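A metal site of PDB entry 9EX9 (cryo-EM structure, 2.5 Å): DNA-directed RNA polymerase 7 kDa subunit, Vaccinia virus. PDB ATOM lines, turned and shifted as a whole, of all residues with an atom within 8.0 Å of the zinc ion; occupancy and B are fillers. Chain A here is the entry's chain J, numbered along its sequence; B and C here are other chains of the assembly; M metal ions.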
ATOM      1  N   VAL A   6      34.005 -14.982  12.725  1.00  0.00           N
ATOM      2  CA  VAL A   6      32.996 -15.769  13.410  1.00  0.00           C
ATOM      3  C   VAL A   6      32.829 -15.234  14.820  1.00  0.00           C
ATOM      4  O   VAL A   6      33.669 -14.480  15.330  1.00  0.00           O
ATOM      5  CB  VAL A   6      33.342 -17.274  13.450  1.00  0.00           C
ATOM      6  CG1 VAL A   6      33.431 -17.835  12.054  1.00  0.00           C
ATOM      7  CG2 VAL A   6      34.643 -17.496  14.186  1.00  0.00           C
ATOM      8  N   CYS A   7      31.726 -15.608  15.459  1.00  0.00           N
ATOM      9  CA  CYS A   7      31.519 -15.319  16.866  1.00  0.00           C
ATOM     10  C   CYS A   7      32.377 -16.246  17.717  1.00  0.00           C
ATOM     11  O   CYS A   7      32.390 -17.464  17.504  1.00  0.00           O
ATOM     12  CB  CYS A   7      30.037 -15.486  17.224  1.00  0.00           C
ATOM     13  SG  CYS A   7      29.648 -15.171  18.947  1.00  0.00           S
ATOM     14  N   SER A   8      33.115 -15.672  18.665  1.00  0.00           N
ATOM     15  CA  SER A   8      34.022 -16.467  19.481  1.00  0.00           C
ATOM     16  C   SER A   8      33.299 -17.333  20.494  1.00  0.00           C
ATOM     17  O   SER A   8      33.910 -18.234  21.077  1.00  0.00           O
ATOM     18  CB  SER A   8      35.003 -15.555  20.203  1.00  0.00           C
ATOM     19  OG  SER A   8      35.502 -14.563  19.342  1.00  0.00           O
ATOM     20  N   THR A   9      32.010 -17.082  20.742  1.00  0.00           N
ATOM     21  CA  THR A   9      31.258 -17.828  21.740  1.00  0.00           C
ATOM     22  C   THR A   9      30.518 -19.012  21.121  1.00  0.00           C
ATOM     23  O   THR A   9      30.576 -20.120  21.665  1.00  0.00           O
ATOM     24  CB  THR A   9      30.270 -16.898  22.447  1.00  0.00           C
ATOM     25  OG1 THR A   9      30.985 -16.022  23.334  1.00  0.00           O
ATOM     26  CG2 THR A   9      29.241 -17.675  23.250  1.00  0.00           C
ATOM     27  N   CYS A  10      29.835 -18.807  19.999  1.00  0.00           N
ATOM     28  CA  CYS A  10      29.066 -19.859  19.370  1.00  0.00           C
ATOM     29  C   CYS A  10      29.591 -20.271  17.999  1.00  0.00           C
ATOM     30  O   CYS A  10      29.146 -21.287  17.465  1.00  0.00           O
ATOM     31  CB  CYS A  10      27.596 -19.427  19.226  1.00  0.00           C
ATOM     32  SG  CYS A  10      27.327 -18.084  18.063  1.00  0.00           S
ATOM     33  N   GLY A  11      30.513 -19.510  17.415  1.00  0.00           N
ATOM     34  CA  GLY A  11      31.099 -19.896  16.152  1.00  0.00           C
ATOM     35  C   GLY A  11      30.293 -19.548  14.918  1.00  0.00           C
ATOM     36  O   GLY A  11      30.623 -20.028  13.833  1.00  0.00           O
ATOM     37  N   LYS A  12      29.271 -18.710  15.041  1.00  0.00           N
ATOM     38  CA  LYS A  12      28.466 -18.335  13.898  1.00  0.00           C
ATOM     39  C   LYS A  12      29.182 -17.315  13.021  1.00  0.00           C
ATOM     40  O   LYS A  12      30.138 -16.668  13.439  1.00  0.00           O
ATOM     41  CB  LYS A  12      27.113 -17.776  14.341  1.00  0.00           C
ATOM     42  CG  LYS A  12      26.042 -18.833  14.516  1.00  0.00           C
ATOM     43  CD  LYS A  12      24.675 -18.211  14.663  1.00  0.00           C
ATOM     44  CE  LYS A  12      23.576 -19.238  14.494  1.00  0.00           C
ATOM     45  NZ  LYS A  12      23.682 -20.347  15.467  1.00  0.00           N
ATOM     46  N   ASP A  13      28.684 -17.179  11.801  1.00  0.00           N
ATOM     47  CA  ASP A  13      29.286 -16.327  10.778  1.00  0.00           C
ATOM     48  C   ASP A  13      28.688 -14.925  10.839  1.00  0.00           C
ATOM     49  O   ASP A  13      27.468 -14.766  10.737  1.00  0.00           O
ATOM     50  CB  ASP A  13      29.059 -16.960   9.408  1.00  0.00           C
ATOM     51  CG  ASP A  13      29.575 -16.123   8.269  1.00  0.00           C
ATOM     52  OD1 ASP A  13      30.197 -15.077   8.519  1.00  0.00           O
ATOM     53  OD2 ASP A  13      29.348 -16.516   7.106  1.00  0.00           O
ATOM     54  N   ILE A  14      29.542 -13.918  11.007  1.00  0.00           N
ATOM     55  CA  ILE A  14      29.076 -12.546  11.178  1.00  0.00           C
ATOM     56  C   ILE A  14      29.778 -11.586  10.219  1.00  0.00           C
ATOM     57  O   ILE A  14      29.840 -10.381  10.484  1.00  0.00           O
ATOM     58  CB  ILE A  14      29.285 -12.076  12.624  1.00  0.00           C
ATOM     59  CG1 ILE A  14      30.768 -12.123  12.990  1.00  0.00           C
ATOM     60  CG2 ILE A  14      28.461 -12.902  13.581  1.00  0.00           C
ATOM     61  CD1 ILE A  14      31.064 -11.651  14.383  1.00  0.00           C
ATOM     62  N   VAL A  35      20.157 -10.827  13.519  1.00  0.00           N
ATOM     63  CA  VAL A  35      21.034 -11.514  14.455  1.00  0.00           C
ATOM     64  C   VAL A  35      20.252 -11.738  15.739  1.00  0.00           C
ATOM     65  O   VAL A  35      19.664 -10.802  16.285  1.00  0.00           O
ATOM     66  CB  VAL A  35      22.305 -10.684  14.735  1.00  0.00           C
ATOM     67  CG1 VAL A  35      23.227 -11.442  15.656  1.00  0.00           C
ATOM     68  CG2 VAL A  35      23.009 -10.362  13.440  1.00  0.00           C
ATOM     69  N   LYS A  36      20.255 -12.977  16.217  1.00  0.00           N
ATOM     70  CA  LYS A  36      19.430 -13.377  17.346  1.00  0.00           C
ATOM     71  C   LYS A  36      20.213 -13.685  18.614  1.00  0.00           C
ATOM     72  O   LYS A  36      19.748 -13.338  19.705  1.00  0.00           O
ATOM     73  CB  LYS A  36      18.600 -14.614  16.981  1.00  0.00           C
ATOM     74  CG  LYS A  36      17.757 -15.155  18.105  1.00  0.00           C
ATOM     75  CD  LYS A  36      16.841 -16.268  17.637  1.00  0.00           C
ATOM     76  CE  LYS A  36      15.960 -16.775  18.758  1.00  0.00           C
ATOM     77  NZ  LYS A  36      15.006 -17.820  18.292  1.00  0.00           N
ATOM     78  N   ASN A  37      21.362 -14.324  18.513  1.00  0.00           N
ATOM     79  CA  ASN A  37      22.077 -14.755  19.713  1.00  0.00           C
ATOM     80  C   ASN A  37      22.698 -13.569  20.441  1.00  0.00           C
ATOM     81  O   ASN A  37      23.202 -12.630  19.828  1.00  0.00           O
ATOM     82  CB  ASN A  37      23.154 -15.764  19.354  1.00  0.00           C
ATOM     83  CG  ASN A  37      22.588 -17.152  19.128  1.00  0.00           C
ATOM     84  OD1 ASN A  37      21.470 -17.439  19.529  1.00  0.00           O
ATOM     85  ND2 ASN A  37      23.371 -18.005  18.498  1.00  0.00           N
ATOM     86  N   GLU A  38      22.671 -13.642  21.771  1.00  0.00           N
ATOM     87  CA  GLU A  38      23.168 -12.548  22.598  1.00  0.00           C
ATOM     88  C   GLU A  38      24.637 -12.274  22.319  1.00  0.00           C
ATOM     89  O   GLU A  38      25.040 -11.128  22.114  1.00  0.00           O
ATOM     90  CB  GLU A  38      22.954 -12.919  24.057  1.00  0.00           C
ATOM     91  CG  GLU A  38      23.394 -11.892  25.054  1.00  0.00           C
ATOM     92  CD  GLU A  38      23.339 -12.418  26.466  1.00  0.00           C
ATOM     93  OE1 GLU A  38      23.800 -13.554  26.680  1.00  0.00           O
ATOM     94  OE2 GLU A  38      22.821 -11.713  27.350  1.00  0.00           O
ATOM     95  N   CYS A  39      25.449 -13.328  22.293  1.00  0.00           N
ATOM     96  CA  CYS A  39      26.880 -13.172  22.051  1.00  0.00           C
ATOM     97  C   CYS A  39      27.146 -12.449  20.738  1.00  0.00           C
ATOM     98  O   CYS A  39      27.983 -11.557  20.665  1.00  0.00           O
ATOM     99  CB  CYS A  39      27.558 -14.531  22.070  1.00  0.00           C
ATOM    100  SG  CYS A  39      26.699 -15.805  21.092  1.00  0.00           S
ATOM    101  N   CYS A  40      26.431 -12.839  19.678  1.00  0.00           N
ATOM    102  CA  CYS A  40      26.658 -12.238  18.369  1.00  0.00           C
ATOM    103  C   CYS A  40      26.308 -10.761  18.368  1.00  0.00           C
ATOM    104  O   CYS A  40      27.019  -9.946  17.781  1.00  0.00           O
ATOM    105  CB  CYS A  40      25.857 -12.991  17.321  1.00  0.00           C
ATOM    106  SG  CYS A  40      26.113 -14.764  17.362  1.00  0.00           S
ATOM    107  N   ARG A  41      25.196 -10.400  19.015  1.00  0.00           N
ATOM    108  CA  ARG A  41      24.829  -8.997  19.091  1.00  0.00           C
ATOM    109  C   ARG A  41      25.892  -8.192  19.827  1.00  0.00           C
ATOM    110  O   ARG A  41      26.291  -7.104  19.372  1.00  0.00           O
ATOM    111  CB  ARG A  41      23.467  -8.862  19.783  1.00  0.00           C
ATOM    112  CG  ARG A  41      22.347  -9.526  19.020  1.00  0.00           C
ATOM    113  CD  ARG A  41      21.091  -9.646  19.863  1.00  0.00           C
ATOM    114  NE  ARG A  41      20.405  -8.382  20.022  1.00  0.00           N
ATOM    115  CZ  ARG A  41      19.552  -7.873  19.155  1.00  0.00           C
ATOM    116  NH1 ARG A  41      19.273  -8.492  18.017  1.00  0.00           N
ATOM    117  NH2 ARG A  41      18.944  -6.721  19.426  1.00  0.00           N
ATOM    118  N   LEU A  42      26.380  -8.705  20.946  1.00  0.00           N
ATOM    119  CA  LEU A  42      27.426  -7.986  21.672  1.00  0.00           C
ATOM    120  C   LEU A  42      28.689  -7.843  20.827  1.00  0.00           C
ATOM    121  O   LEU A  42      29.318  -6.778  20.820  1.00  0.00           O
ATOM    122  CB  LEU A  42      27.739  -8.677  22.985  1.00  0.00           C
ATOM    123  CG  LEU A  42      26.866  -8.335  24.192  1.00  0.00           C
ATOM    124  CD1 LEU A  42      27.296  -9.145  25.385  1.00  0.00           C
ATOM    125  CD2 LEU A  42      26.934  -6.859  24.518  1.00  0.00           C
ATOM    126  N   LYS A  43      29.075  -8.900  20.117  1.00  0.00           N
ATOM    127  CA  LYS A  43      30.282  -8.827  19.302  1.00  0.00           C
ATOM    128  C   LYS A  43      30.133  -7.782  18.201  1.00  0.00           C
ATOM    129  O   LYS A  43      31.041  -6.975  17.984  1.00  0.00           O
ATOM    130  CB  LYS A  43      30.601 -10.192  18.698  1.00  0.00           C
ATOM    131  CG  LYS A  43      30.958 -11.246  19.723  1.00  0.00           C
ATOM    132  CD  LYS A  43      32.311 -10.994  20.334  1.00  0.00           C
ATOM    133  CE  LYS A  43      32.365 -11.524  21.747  1.00  0.00           C
ATOM    134  NZ  LYS A  43      32.094 -12.978  21.793  1.00  0.00           N
ATOM    135  N   THR B 743      30.659 -15.097  27.858  1.00  0.00           N
ATOM    136  CA  THR B 743      29.506 -15.693  28.531  1.00  0.00           C
ATOM    137  C   THR B 743      29.974 -16.535  29.704  1.00  0.00           C
ATOM    138  O   THR B 743      30.886 -17.358  29.552  1.00  0.00           O
ATOM    139  CB  THR B 743      28.709 -16.553  27.547  1.00  0.00           C
ATOM    140  OG1 THR B 743      28.263 -15.741  26.451  1.00  0.00           O
ATOM    141  CG2 THR B 743      27.506 -17.158  28.229  1.00  0.00           C
ATOM    142  N   ILE B 909      23.628 -22.753  23.710  1.00  0.00           N
ATOM    143  CA  ILE B 909      24.752 -21.900  24.062  1.00  0.00           C
ATOM    144  C   ILE B 909      25.464 -22.511  25.260  1.00  0.00           C
ATOM    145  O   ILE B 909      24.837 -22.750  26.301  1.00  0.00           O
ATOM    146  CB  ILE B 909      24.306 -20.461  24.357  1.00  0.00           C
ATOM    147  CG1 ILE B 909      23.449 -19.910  23.214  1.00  0.00           C
ATOM    148  CG2 ILE B 909      25.503 -19.578  24.600  1.00  0.00           C
ATOM    149  CD1 ILE B 909      24.146 -19.861  21.883  1.00  0.00           C
ATOM    150  N   GLU C   7      19.316 -17.474   9.768  1.00  0.00           N
ATOM    151  CA  GLU C   7      19.446 -18.498  10.796  1.00  0.00           C
ATOM    152  C   GLU C   7      18.157 -19.312  10.863  1.00  0.00           C
ATOM    153  O   GLU C   7      17.064 -18.742  10.840  1.00  0.00           O
ATOM    154  CB  GLU C   7      19.741 -17.854  12.149  1.00  0.00           C
ATOM    155  CG  GLU C   7      20.906 -16.883  12.137  1.00  0.00           C
ATOM    156  CD  GLU C   7      21.115 -16.213  13.471  1.00  0.00           C
ATOM    157  OE1 GLU C   7      20.162 -16.180  14.275  1.00  0.00           O
ATOM    158  OE2 GLU C   7      22.233 -15.720  13.737  1.00  0.00           O
ATOM    159  N   ILE C 188      25.201 -26.459  14.752  1.00  0.00           N
ATOM    160  CA  ILE C 188      25.029 -26.818  16.156  1.00  0.00           C
ATOM    161  C   ILE C 188      23.902 -27.833  16.282  1.00  0.00           C
ATOM    162  O   ILE C 188      22.877 -27.722  15.613  1.00  0.00           O
ATOM    163  CB  ILE C 188      24.752 -25.576  17.029  1.00  0.00           C
ATOM    164  CG1 ILE C 188      25.945 -24.628  16.973  1.00  0.00           C
ATOM    165  CG2 ILE C 188      24.493 -25.999  18.471  1.00  0.00           C
ATOM    166  CD1 ILE C 188      25.745 -23.337  17.726  1.00  0.00           C
HETATM  167 ZN    ZN M   1      27.441 -15.912  18.890  1.00  0.00          ZN
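The zinc ion is bound by the side-chain sulfur (SG) of Cys 39, the side-chain sulfur (SG) of Cys 40, the side-chain sulfur (SG) of Cys 10 and the side-chain sulfur (SG) of Cys 7 of chain A.
The zinc ion has four donor atoms within binding distance.
Of the 22 residues printed, 4 come within 4 Å of the zinc ion.
The nearest printed residue that does not touch the zinc ion is Asn 37 (4.3 Å).
The backbone NH (N) of Lys 12 lies close to the side-chain sulfur (SG) of Cys 10, at 3.6 Å.
The backbone NH (N) of Cys 7 of chain A is in hydrogen-bond range of the backbone carbonyl oxygen (O) of Lys 12 (2.8 Å).
The side-chain sulfur (SG) of Cys 7 of chain A lies close to the backbone NH (N) of Thr 9 (3.5 Å).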
